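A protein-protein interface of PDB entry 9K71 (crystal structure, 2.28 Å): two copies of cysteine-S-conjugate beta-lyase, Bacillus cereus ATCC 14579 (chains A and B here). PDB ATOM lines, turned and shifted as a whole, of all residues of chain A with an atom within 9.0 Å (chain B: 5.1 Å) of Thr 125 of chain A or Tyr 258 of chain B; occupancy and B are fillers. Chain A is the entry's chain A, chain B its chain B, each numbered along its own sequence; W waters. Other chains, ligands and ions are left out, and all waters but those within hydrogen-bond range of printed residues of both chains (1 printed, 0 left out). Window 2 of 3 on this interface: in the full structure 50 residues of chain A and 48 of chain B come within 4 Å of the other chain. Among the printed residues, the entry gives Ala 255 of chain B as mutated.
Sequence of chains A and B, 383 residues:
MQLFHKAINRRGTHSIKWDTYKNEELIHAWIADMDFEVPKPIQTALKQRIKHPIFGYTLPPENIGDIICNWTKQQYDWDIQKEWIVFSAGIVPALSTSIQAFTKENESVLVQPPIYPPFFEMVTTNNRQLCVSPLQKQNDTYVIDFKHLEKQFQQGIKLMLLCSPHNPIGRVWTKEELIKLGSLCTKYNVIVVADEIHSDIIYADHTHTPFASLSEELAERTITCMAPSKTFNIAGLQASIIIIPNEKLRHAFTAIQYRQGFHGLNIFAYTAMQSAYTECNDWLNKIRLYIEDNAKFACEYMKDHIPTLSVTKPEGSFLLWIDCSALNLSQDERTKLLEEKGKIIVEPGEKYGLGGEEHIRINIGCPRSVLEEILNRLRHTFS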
ATOM      1  N   VAL A  92      -9.683 -21.621 -15.968  1.00  0.00           N
ATOM      2  CA  VAL A  92      -8.362 -21.405 -16.559  1.00  0.00           C
ATOM      3  C   VAL A  92      -7.890 -22.677 -17.239  1.00  0.00           C
ATOM      4  O   VAL A  92      -7.401 -22.602 -18.383  1.00  0.00           O
ATOM      5  CB  VAL A  92      -7.389 -20.850 -15.504  1.00  0.00           C
ATOM      6  CG1 VAL A  92      -5.936 -20.824 -15.982  1.00  0.00           C
ATOM      7  CG2 VAL A  92      -7.791 -19.441 -15.135  1.00  0.00           C
ATOM      8  N   PRO A  93      -8.029 -23.868 -16.641  1.00  0.00           N
ATOM      9  CA  PRO A  93      -7.753 -25.095 -17.408  1.00  0.00           C
ATOM     10  C   PRO A  93      -8.663 -25.258 -18.624  1.00  0.00           C
ATOM     11  O   PRO A  93      -8.270 -25.901 -19.609  1.00  0.00           O
ATOM     12  CB  PRO A  93      -7.957 -26.218 -16.373  1.00  0.00           C
ATOM     13  CG  PRO A  93      -7.813 -25.522 -15.003  1.00  0.00           C
ATOM     14  CD  PRO A  93      -8.409 -24.162 -15.246  1.00  0.00           C
ATOM     15  N   SER A  96      -6.791 -23.267 -21.343  1.00  0.00           N
ATOM     16  CA  SER A  96      -5.618 -24.019 -21.760  1.00  0.00           C
ATOM     17  C   SER A  96      -6.019 -25.266 -22.543  1.00  0.00           C
ATOM     18  O   SER A  96      -5.394 -25.601 -23.556  1.00  0.00           O
ATOM     19  CB  SER A  96      -4.792 -24.389 -20.533  1.00  0.00           C
ATOM     20  OG  SER A  96      -3.990 -25.504 -20.817  1.00  0.00           O
ATOM     21  N   THR A  97      -7.034 -25.990 -22.069  1.00  0.00           N
ATOM     22  CA  THR A  97      -7.571 -27.106 -22.849  1.00  0.00           C
ATOM     23  C   THR A  97      -8.029 -26.638 -24.238  1.00  0.00           C
ATOM     24  O   THR A  97      -7.692 -27.269 -25.250  1.00  0.00           O
ATOM     25  CB  THR A  97      -8.686 -27.792 -22.055  1.00  0.00           C
ATOM     26  OG1 THR A  97      -8.146 -28.233 -20.793  1.00  0.00           O
ATOM     27  CG2 THR A  97      -9.265 -28.966 -22.796  1.00  0.00           C
ATOM     28  N   ILE A  99      -7.048 -23.920 -25.939  1.00  0.00           N
ATOM     29  CA  ILE A  99      -5.871 -23.599 -26.737  1.00  0.00           C
ATOM     30  C   ILE A  99      -5.299 -24.868 -27.341  1.00  0.00           C
ATOM     31  O   ILE A  99      -4.947 -24.906 -28.529  1.00  0.00           O
ATOM     32  CB  ILE A  99      -4.816 -22.865 -25.893  1.00  0.00           C
ATOM     33  CG1 ILE A  99      -5.391 -21.543 -25.399  1.00  0.00           C
ATOM     34  CG2 ILE A  99      -3.587 -22.583 -26.739  1.00  0.00           C
ATOM     35  CD1 ILE A  99      -4.642 -20.943 -24.282  1.00  0.00           C
ATOM     36  N   GLN A 100      -5.191 -25.925 -26.550  1.00  0.00           N
ATOM     37  CA  GLN A 100      -4.545 -27.164 -27.044  1.00  0.00           C
ATOM     38  C   GLN A 100      -5.459 -27.895 -28.024  1.00  0.00           C
ATOM     39  O   GLN A 100      -4.959 -28.308 -29.045  1.00  0.00           O
ATOM     40  CB  GLN A 100      -4.109 -28.034 -25.871  1.00  0.00           C
ATOM     41  CG  GLN A 100      -2.843 -27.520 -25.205  1.00  0.00           C
ATOM     42  CD  GLN A 100      -2.349 -28.404 -24.090  1.00  0.00           C
ATOM     43  OE1 GLN A 100      -2.427 -29.625 -24.154  1.00  0.00           O
ATOM     44  NE2 GLN A 100      -1.824 -27.785 -23.049  1.00  0.00           N
ATOM     45  N   GLU A 105       0.684 -25.654 -32.286  1.00  0.00           N
ATOM     46  CA  GLU A 105       1.775 -24.804 -31.831  1.00  0.00           C
ATOM     47  C   GLU A 105       2.046 -23.715 -32.870  1.00  0.00           C
ATOM     48  O   GLU A 105       1.881 -23.930 -34.073  1.00  0.00           O
ATOM     49  CB  GLU A 105       3.023 -25.651 -31.562  1.00  0.00           C
ATOM     50  CG  GLU A 105       3.417 -25.734 -30.081  1.00  0.00           C
ATOM     51  CD  GLU A 105       4.681 -26.541 -29.855  1.00  0.00           C
ATOM     52  OE1 GLU A 105       4.559 -27.750 -29.561  1.00  0.00           O
ATOM     53  OE2 GLU A 105       5.797 -25.982 -29.983  1.00  0.00           O
ATOM     54  N   PRO A 117      -4.894 -11.611 -16.488  1.00  0.00           N
ATOM     55  CA  PRO A 117      -3.614 -12.009 -17.115  1.00  0.00           C
ATOM     56  C   PRO A 117      -3.561 -13.466 -17.563  1.00  0.00           C
ATOM     57  O   PRO A 117      -2.939 -13.745 -18.600  1.00  0.00           O
ATOM     58  CB  PRO A 117      -2.578 -11.708 -16.020  1.00  0.00           C
ATOM     59  CG  PRO A 117      -3.208 -10.675 -15.176  1.00  0.00           C
ATOM     60  CD  PRO A 117      -4.685 -10.978 -15.170  1.00  0.00           C
ATOM     61  N   PRO A 118      -4.163 -14.431 -16.841  1.00  0.00           N
ATOM     62  CA  PRO A 118      -4.108 -15.828 -17.330  1.00  0.00           C
ATOM     63  C   PRO A 118      -4.474 -15.993 -18.783  1.00  0.00           C
ATOM     64  O   PRO A 118      -4.008 -16.947 -19.425  1.00  0.00           O
ATOM     65  CB  PRO A 118      -5.114 -16.543 -16.418  1.00  0.00           C
ATOM     66  CG  PRO A 118      -4.906 -15.868 -15.114  1.00  0.00           C
ATOM     67  CD  PRO A 118      -4.668 -14.395 -15.449  1.00  0.00           C
ATOM     68  N   PHE A 119      -5.267 -15.059 -19.334  1.00  0.00           N
ATOM     69  CA  PHE A 119      -5.482 -15.016 -20.774  1.00  0.00           C
ATOM     70  C   PHE A 119      -4.149 -14.963 -21.492  1.00  0.00           C
ATOM     71  O   PHE A 119      -3.932 -15.681 -22.473  1.00  0.00           O
ATOM     72  CB  PHE A 119      -6.331 -13.798 -21.168  1.00  0.00           C
ATOM     73  CG  PHE A 119      -7.798 -13.996 -20.959  1.00  0.00           C
ATOM     74  CD1 PHE A 119      -8.288 -14.383 -19.713  1.00  0.00           C
ATOM     75  CD2 PHE A 119      -8.697 -13.809 -22.012  1.00  0.00           C
ATOM     76  CE1 PHE A 119      -9.636 -14.579 -19.520  1.00  0.00           C
ATOM     77  CE2 PHE A 119     -10.051 -13.989 -21.824  1.00  0.00           C
ATOM     78  CZ  PHE A 119     -10.525 -14.380 -20.581  1.00  0.00           C
ATOM     79  N   PHE A 120      -3.231 -14.126 -20.992  1.00  0.00           N
ATOM     80  CA  PHE A 120      -1.906 -14.013 -21.590  1.00  0.00           C
ATOM     81  C   PHE A 120      -1.096 -15.282 -21.359  1.00  0.00           C
ATOM     82  O   PHE A 120      -0.429 -15.782 -22.273  1.00  0.00           O
ATOM     83  CB  PHE A 120      -1.152 -12.822 -20.989  1.00  0.00           C
ATOM     84  CG  PHE A 120      -1.822 -11.477 -21.173  1.00  0.00           C
ATOM     85  CD1 PHE A 120      -1.864 -10.872 -22.407  1.00  0.00           C
ATOM     86  CD2 PHE A 120      -2.336 -10.790 -20.088  1.00  0.00           C
ATOM     87  CE1 PHE A 120      -2.438  -9.630 -22.566  1.00  0.00           C
ATOM     88  CE2 PHE A 120      -2.925  -9.511 -20.241  1.00  0.00           C
ATOM     89  CZ  PHE A 120      -2.970  -8.951 -21.476  1.00  0.00           C
ATOM     90  N   GLU A 121      -1.142 -15.791 -20.129  1.00  0.00           N
ATOM     91  CA  GLU A 121      -0.206 -16.804 -19.661  1.00  0.00           C
ATOM     92  C   GLU A 121      -0.449 -18.182 -20.289  1.00  0.00           C
ATOM     93  O   GLU A 121       0.501 -18.840 -20.719  1.00  0.00           O
ATOM     94  CB  GLU A 121      -0.275 -16.854 -18.141  1.00  0.00           C
ATOM     95  CG  GLU A 121       0.418 -15.705 -17.501  1.00  0.00           C
ATOM     96  CD  GLU A 121       1.920 -15.815 -17.631  1.00  0.00           C
ATOM     97  OE1 GLU A 121       2.475 -16.892 -17.265  1.00  0.00           O
ATOM     98  OE2 GLU A 121       2.548 -14.830 -18.092  1.00  0.00           O
ATOM     99  N   MET A 122      -1.704 -18.626 -20.365  1.00  0.00           N
ATOM    100  CA  MET A 122      -1.979 -19.953 -20.919  1.00  0.00           C
ATOM    101  C   MET A 122      -1.705 -19.994 -22.414  1.00  0.00           C
ATOM    102  O   MET A 122      -1.412 -21.065 -22.963  1.00  0.00           O
ATOM    103  CB  MET A 122      -3.409 -20.381 -20.632  1.00  0.00           C
ATOM    104  CG  MET A 122      -3.792 -20.462 -19.158  1.00  0.00           C
ATOM    105  SD  MET A 122      -2.723 -21.536 -18.214  1.00  0.00           S
ATOM    106  CE  MET A 122      -1.578 -20.416 -17.377  1.00  0.00           C
ATOM    107  N   VAL A 123      -1.764 -18.841 -23.083  1.00  0.00           N
ATOM    108  CA  VAL A 123      -1.344 -18.782 -24.480  1.00  0.00           C
ATOM    109  C   VAL A 123       0.162 -18.982 -24.611  1.00  0.00           C
ATOM    110  O   VAL A 123       0.622 -19.870 -25.338  1.00  0.00           O
ATOM    111  CB  VAL A 123      -1.752 -17.451 -25.121  1.00  0.00           C
ATOM    112  CG1 VAL A 123      -1.134 -17.351 -26.506  1.00  0.00           C
ATOM    113  CG2 VAL A 123      -3.252 -17.312 -25.125  1.00  0.00           C
ATOM    114  N   THR A 124       0.957 -18.113 -23.968  1.00  0.00           N
ATOM    115  CA  THR A 124       2.396 -18.162 -24.223  1.00  0.00           C
ATOM    116  C   THR A 124       3.015 -19.407 -23.616  1.00  0.00           C
ATOM    117  O   THR A 124       3.899 -20.013 -24.226  1.00  0.00           O
ATOM    118  CB  THR A 124       3.105 -16.917 -23.705  1.00  0.00           C
ATOM    119  OG1 THR A 124       3.217 -16.968 -22.271  1.00  0.00           O
ATOM    120  CG2 THR A 124       2.370 -15.647 -24.184  1.00  0.00           C
ATOM    121  N   THR A 125       2.572 -19.812 -22.422  1.00  0.00           N
ATOM    122  CA  THR A 125       3.153 -21.033 -21.882  1.00  0.00           C
ATOM    123  C   THR A 125       2.795 -22.268 -22.706  1.00  0.00           C
ATOM    124  O   THR A 125       3.415 -23.308 -22.507  1.00  0.00           O
ATOM    125  CB  THR A 125       2.753 -21.212 -20.419  1.00  0.00           C
ATOM    126  OG1 THR A 125       1.326 -21.305 -20.299  1.00  0.00           O
ATOM    127  CG2 THR A 125       3.282 -20.002 -19.583  1.00  0.00           C
ATOM    128  N   ASN A 126       1.872 -22.164 -23.673  1.00  0.00           N
ATOM    129  CA  ASN A 126       1.544 -23.271 -24.570  1.00  0.00           C
ATOM    130  C   ASN A 126       2.130 -23.097 -25.960  1.00  0.00           C
ATOM    131  O   ASN A 126       1.825 -23.897 -26.856  1.00  0.00           O
ATOM    132  CB  ASN A 126       0.030 -23.436 -24.687  1.00  0.00           C
ATOM    133  CG  ASN A 126      -0.538 -24.324 -23.628  1.00  0.00           C
ATOM    134  OD1 ASN A 126      -0.272 -25.530 -23.598  1.00  0.00           O
ATOM    135  ND2 ASN A 126      -1.351 -23.748 -22.752  1.00  0.00           N
ATOM    136  N   ASN A 127       3.008 -22.107 -26.141  1.00  0.00           N
ATOM    137  CA  ASN A 127       3.710 -21.869 -27.402  1.00  0.00           C
ATOM    138  C   ASN A 127       2.752 -21.501 -28.542  1.00  0.00           C
ATOM    139  O   ASN A 127       3.050 -21.714 -29.716  1.00  0.00           O
ATOM    140  CB  ASN A 127       4.586 -23.073 -27.793  1.00  0.00           C
ATOM    141  CG  ASN A 127       5.523 -22.767 -28.975  1.00  0.00           C
ATOM    142  OD1 ASN A 127       5.463 -23.424 -30.014  1.00  0.00           O
ATOM    143  ND2 ASN A 127       6.340 -21.728 -28.836  1.00  0.00           N
ATOM    144  N   ARG A 128       1.600 -20.924 -28.236  1.00  0.00           N
ATOM    145  CA  ARG A 128       0.788 -20.349 -29.301  1.00  0.00           C
ATOM    146  C   ARG A 128       1.143 -18.866 -29.443  1.00  0.00           C
ATOM    147  O   ARG A 128       1.639 -18.239 -28.508  1.00  0.00           O
ATOM    148  CB  ARG A 128      -0.703 -20.514 -29.004  1.00  0.00           C
ATOM    149  CG  ARG A 128      -1.320 -21.802 -29.537  1.00  0.00           C
ATOM    150  CD  ARG A 128      -0.727 -23.008 -28.833  1.00  0.00           C
ATOM    151  NE  ARG A 128      -1.406 -24.225 -29.235  1.00  0.00           N
ATOM    152  CZ  ARG A 128      -1.065 -25.450 -28.855  1.00  0.00           C
ATOM    153  NH1 ARG A 128      -0.026 -25.655 -28.044  1.00  0.00           N
ATOM    154  NH2 ARG A 128      -1.778 -26.475 -29.295  1.00  0.00           N
ATOM    155  N   GLN A 129       0.961 -18.319 -30.632  1.00  0.00           N
ATOM    156  CA  GLN A 129       1.289 -16.910 -30.818  1.00  0.00           C
ATOM    157  C   GLN A 129       0.185 -16.060 -30.191  1.00  0.00           C
ATOM    158  O   GLN A 129      -0.986 -16.220 -30.531  1.00  0.00           O
ATOM    159  CB  GLN A 129       1.486 -16.577 -32.298  1.00  0.00           C
ATOM    160  CG  GLN A 129       1.777 -15.079 -32.533  1.00  0.00           C
ATOM    161  CD  GLN A 129       2.312 -14.761 -33.935  1.00  0.00           C
ATOM    162  OE1 GLN A 129       2.566 -15.657 -34.742  1.00  0.00           O
ATOM    163  NE2 GLN A 129       2.502 -13.478 -34.214  1.00  0.00           N
ATOM    164  N   LEU A 130       0.546 -15.204 -29.238  1.00  0.00           N
ATOM    165  CA  LEU A 130      -0.426 -14.354 -28.552  1.00  0.00           C
ATOM    166  C   LEU A 130      -0.629 -13.081 -29.358  1.00  0.00           C
ATOM    167  O   LEU A 130       0.326 -12.313 -29.542  1.00  0.00           O
ATOM    168  CB  LEU A 130       0.049 -14.000 -27.142  1.00  0.00           C
ATOM    169  CG  LEU A 130      -0.784 -12.951 -26.429  1.00  0.00           C
ATOM    170  CD1 LEU A 130      -2.204 -13.495 -26.200  1.00  0.00           C
ATOM    171  CD2 LEU A 130      -0.111 -12.572 -25.131  1.00  0.00           C
ATOM    172  N   THR B 254       6.235 -28.886 -12.921  1.00  0.00           N
ATOM    173  CA  THR B 254       5.394 -27.769 -12.511  1.00  0.00           C
ATOM    174  C   THR B 254       5.062 -26.882 -13.700  1.00  0.00           C
ATOM    175  O   THR B 254       3.933 -26.386 -13.801  1.00  0.00           O
ATOM    176  CB  THR B 254       6.105 -26.940 -11.426  1.00  0.00           C
ATOM    177  OG1 THR B 254       7.466 -26.744 -11.813  1.00  0.00           O
ATOM    178  CG2 THR B 254       6.133 -27.671 -10.148  1.00  0.00           C
ATOM    179  N   ALA B 255       5.977 -26.796 -14.666  1.00  0.00           N
ATOM    180  CA  ALA B 255       5.726 -26.026 -15.875  1.00  0.00           C
ATOM    181  C   ALA B 255       4.625 -26.643 -16.751  1.00  0.00           C
ATOM    182  O   ALA B 255       3.909 -25.913 -17.445  1.00  0.00           O
ATOM    183  CB  ALA B 255       7.044 -25.855 -16.652  1.00  0.00           C
ATOM    184  N   ILE B 256       4.443 -27.964 -16.723  1.00  0.00           N
ATOM    185  CA  ILE B 256       3.369 -28.559 -17.518  1.00  0.00           C
ATOM    186  C   ILE B 256       2.005 -28.293 -16.877  1.00  0.00           C
ATOM    187  O   ILE B 256       1.031 -27.959 -17.563  1.00  0.00           O
ATOM    188  CB  ILE B 256       3.587 -30.070 -17.706  1.00  0.00           C
ATOM    189  CG1 ILE B 256       4.988 -30.409 -18.241  1.00  0.00           C
ATOM    190  CG2 ILE B 256       2.465 -30.626 -18.568  1.00  0.00           C
ATOM    191  CD1 ILE B 256       5.334 -29.897 -19.619  1.00  0.00           C
ATOM    192  N   GLN B 257       1.902 -28.502 -15.563  1.00  0.00           N
ATOM    193  CA  GLN B 257       0.659 -28.228 -14.851  1.00  0.00           C
ATOM    194  C   GLN B 257       0.237 -26.769 -15.005  1.00  0.00           C
ATOM    195  O   GLN B 257      -0.957 -26.471 -15.205  1.00  0.00           O
ATOM    196  CB  GLN B 257       0.829 -28.522 -13.372  1.00  0.00           C
ATOM    197  CG  GLN B 257       1.464 -29.835 -12.982  1.00  0.00           C
ATOM    198  CD  GLN B 257       1.319 -30.002 -11.497  1.00  0.00           C
ATOM    199  OE1 GLN B 257       1.899 -29.243 -10.719  1.00  0.00           O
ATOM    200  NE2 GLN B 257       0.466 -30.925 -11.091  1.00  0.00           N
ATOM    201  N   TYR B 258       1.206 -25.849 -14.863  1.00  0.00           N
ATOM    202  CA  TYR B 258       0.920 -24.429 -15.007  1.00  0.00           C
ATOM    203  C   TYR B 258       0.339 -24.120 -16.386  1.00  0.00           C
ATOM    204  O   TYR B 258      -0.647 -23.392 -16.491  1.00  0.00           O
ATOM    205  CB  TYR B 258       2.177 -23.604 -14.761  1.00  0.00           C
ATOM    206  CG  TYR B 258       1.926 -22.082 -14.829  1.00  0.00           C
ATOM    207  CD1 TYR B 258       1.237 -21.424 -13.818  1.00  0.00           C
ATOM    208  CD2 TYR B 258       2.367 -21.319 -15.926  1.00  0.00           C
ATOM    209  CE1 TYR B 258       0.981 -20.029 -13.892  1.00  0.00           C
ATOM    210  CE2 TYR B 258       2.127 -19.936 -16.000  1.00  0.00           C
ATOM    211  CZ  TYR B 258       1.433 -19.307 -14.978  1.00  0.00           C
ATOM    212  OH  TYR B 258       1.203 -17.956 -15.039  1.00  0.00           O
ATOM    213  N   ARG B 259       0.919 -24.675 -17.461  1.00  0.00           N
ATOM    214  CA  ARG B 259       0.378 -24.353 -18.779  1.00  0.00           C
ATOM    215  C   ARG B 259      -0.961 -25.008 -19.023  1.00  0.00           C
ATOM    216  O   ARG B 259      -1.692 -24.564 -19.915  1.00  0.00           O
ATOM    217  CB  ARG B 259       1.323 -24.741 -19.899  1.00  0.00           C
ATOM    218  CG  ARG B 259       1.354 -26.212 -20.190  1.00  0.00           C
ATOM    219  CD  ARG B 259       2.159 -26.421 -21.423  1.00  0.00           C
ATOM    220  NE  ARG B 259       2.104 -27.791 -21.881  1.00  0.00           N
ATOM    221  CZ  ARG B 259       3.050 -28.352 -22.629  1.00  0.00           C
ATOM    222  NH1 ARG B 259       4.120 -27.643 -22.974  1.00  0.00           N
ATOM    223  NH2 ARG B 259       2.923 -29.617 -23.035  1.00  0.00           N
ATOM    224  N   GLN B 260      -1.303 -26.030 -18.243  1.00  0.00           N
ATOM    225  CA  GLN B 260      -2.634 -26.606 -18.240  1.00  0.00           C
ATOM    226  C   GLN B 260      -3.567 -25.934 -17.238  1.00  0.00           C
ATOM    227  O   GLN B 260      -4.633 -26.486 -16.938  1.00  0.00           O
ATOM    228  CB  GLN B 260      -2.545 -28.110 -17.959  1.00  0.00           C
ATOM    229  CG  GLN B 260      -1.801 -28.815 -19.068  1.00  0.00           C
ATOM    230  CD  GLN B 260      -1.348 -30.204 -18.690  1.00  0.00           C
ATOM    231  OE1 GLN B 260      -1.768 -30.759 -17.661  1.00  0.00           O
ATOM    232  NE2 GLN B 260      -0.500 -30.790 -19.539  1.00  0.00           N
ATOM    233  N   GLY B 261      -3.194 -24.766 -16.724  1.00  0.00           N
ATOM    234  CA  GLY B 261      -4.050 -23.996 -15.848  1.00  0.00           C
ATOM    235  C   GLY B 261      -4.186 -24.512 -14.434  1.00  0.00           C
ATOM    236  O   GLY B 261      -5.042 -24.004 -13.703  1.00  0.00           O
ATOM    237  N   PHE B 262      -3.343 -25.468 -14.014  1.00  0.00           N
ATOM    238  CA  PHE B 262      -3.419 -26.033 -12.667  1.00  0.00           C
ATOM    239  C   PHE B 262      -2.972 -25.014 -11.628  1.00  0.00           C
ATOM    240  O   PHE B 262      -1.946 -24.345 -11.797  1.00  0.00           O
ATOM    241  CB  PHE B 262      -2.544 -27.282 -12.545  1.00  0.00           C
ATOM    242  CG  PHE B 262      -2.542 -27.922 -11.152  1.00  0.00           C
ATOM    243  CD1 PHE B 262      -3.651 -28.599 -10.674  1.00  0.00           C
ATOM    244  CD2 PHE B 262      -1.406 -27.859 -10.339  1.00  0.00           C
ATOM    245  CE1 PHE B 262      -3.640 -29.191  -9.391  1.00  0.00           C
ATOM    246  CE2 PHE B 262      -1.387 -28.449  -9.046  1.00  0.00           C
ATOM    247  CZ  PHE B 262      -2.498 -29.130  -8.585  1.00  0.00           C
ATOM    248  N   HIS B 263      -3.766 -24.895 -10.566  1.00  0.00           N
ATOM    249  CA  HIS B 263      -3.531 -23.985  -9.460  1.00  0.00           C
ATOM    250  C   HIS B 263      -3.813 -24.678  -8.138  1.00  0.00           C
ATOM    251  O   HIS B 263      -4.412 -24.092  -7.231  1.00  0.00           O
ATOM    252  CB  HIS B 263      -4.362 -22.703  -9.600  1.00  0.00           C
ATOM    253  CG  HIS B 263      -4.064 -21.925 -10.848  1.00  0.00           C
ATOM    254  ND1 HIS B 263      -2.788 -21.785 -11.352  1.00  0.00           N
ATOM    255  CD2 HIS B 263      -4.877 -21.248 -11.697  1.00  0.00           C
ATOM    256  CE1 HIS B 263      -2.826 -21.055 -12.455  1.00  0.00           C
ATOM    257  NE2 HIS B 263      -4.081 -20.710 -12.683  1.00  0.00           N
HETATM  258  O   HOH W   1      -5.547 -27.841 -19.557  1.00  0.00           O
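The side-chain hydroxyl (OG) of Ser 96 of chain A lies within hydrogen-bond range of the backbone carbonyl oxygen (O) of Arg 259 of chain B (2.6 Å).
The side-chain carboxylate of Glu 121 of chain A is in hydrogen-bond range of the side-chain hydroxyl of Tyr 258 of chain B, 2.8 Å away.
SD of Met 122 of chain A is in hydrogen-bond range of N of Gly 261 of chain B, at 3.6 Å.
ND2 of Asn 126 of chain A sits at hydrogen-bond distance from O of Arg 259 of chain B (3.0 Å).
The side-chain sulfur of Met 122 of chain A sits close to the backbone carbonyl oxygen of Tyr 258 of chain B.
The side-chain sulfur (SD) of Met 122 of chain A lies close to the backbone carbonyl oxygen (O) of Arg 259 of chain B, at 3.6 Å.
OG1 of Thr 97 of chain A sits at hydrogen-bond distance from O of Pro 93 of chain A, 2.6 Å away.
The side-chain amide nitrogen of Gln 100 of chain A is in hydrogen-bond range of the side-chain amide oxygen of Asn 126 of chain A.
The backbone carbonyl oxygen of Glu 121 of chain A sits at hydrogen-bond distance from the side-chain hydroxyl of Thr 125 of chain A (2.6 Å).
The backbone carbonyl oxygen (O) of Met 122 of chain A sits at hydrogen-bond distance from the side-chain amide nitrogen (ND2) of Asn 126 of chain A (2.7 Å).
NH1 of Arg 128 of chain A sits at hydrogen-bond distance from O of Asn 126 of chain A.
CG1 of Val 92 of chain A touches CA of Gly 261 of chain B, at 3.7 Å.
CG1 of Val 92 of chain A touches NE2 of His 263 of chain B, at 3.8 Å.
Pro 93 of chain A touches Gln 260 of chain B.
Pro 93 of chain A touches Gly 261 of chain B (CG to O, 3.4 Å).
Gln 260 of chain B touches Ser 96 of chain A (CA to OG, 3.1 Å).
Tyr 258 of chain B touches Thr 125 of chain A (CE2 to CG2, 3.8 Å).
OG1 of Thr 125 of chain A touches CB of Arg 259 of chain B (3.5 Å).
Pro 117 of chain A touches none of the printed residues of chain B.
Of the printed residues of chain B, Glu 121 of chain A touches Tyr 258.
Thr 125 of chain A touches two residues of chain B.
Printed residues of chain B within 4 Å of Asn 126 of chain A: Arg 259.
Of chain A, only Glu 121 (2.8 Å), Met 122 (3.2 Å) and Thr 125 (3.8 Å) come within 4 Å of Tyr 258 of chain B.
Of the printed residues of chain A, Arg 259 of chain B touches Ser 96, Met 122, Thr 125 and Asn 126.
The nearest printed residue of chain B that does not touch Thr 125 of chain A is Ala 255 of chain B (5.7 Å).
The nearest residue of chain A that does not touch Tyr 258 of chain B is Ser 96 of chain A (5.9 Å).
Hydrophobic or aromatic side chains of chain B that line the printed part of chain A: Tyr 258 and His 263.
Hydrophobic or aromatic side chains of chain A within 4 Å of the printed part of chain B: Val 92, Pro 93 and Met 122.
Among the printed residues, no Asp or Glu carboxylate lies within 4 Å of a Lys or Arg side-chain nitrogen of the other chain.
No position is printed for both chains.
Of the 13 pairs that touch across the chains among the printed residues, none has its exchanged pair printed and touching as well.
Water W1 lies within hydrogen-bond range of the side-chain hydroxyl (OG1) of Thr 97 of chain A, the side-chain hydroxyl (OG) of Ser 96 of chain A, the backbone carbonyl oxygen (O) of Gln 260 of chain B and the backbone carbonyl oxygen (O) of Pro 93 of chain A.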
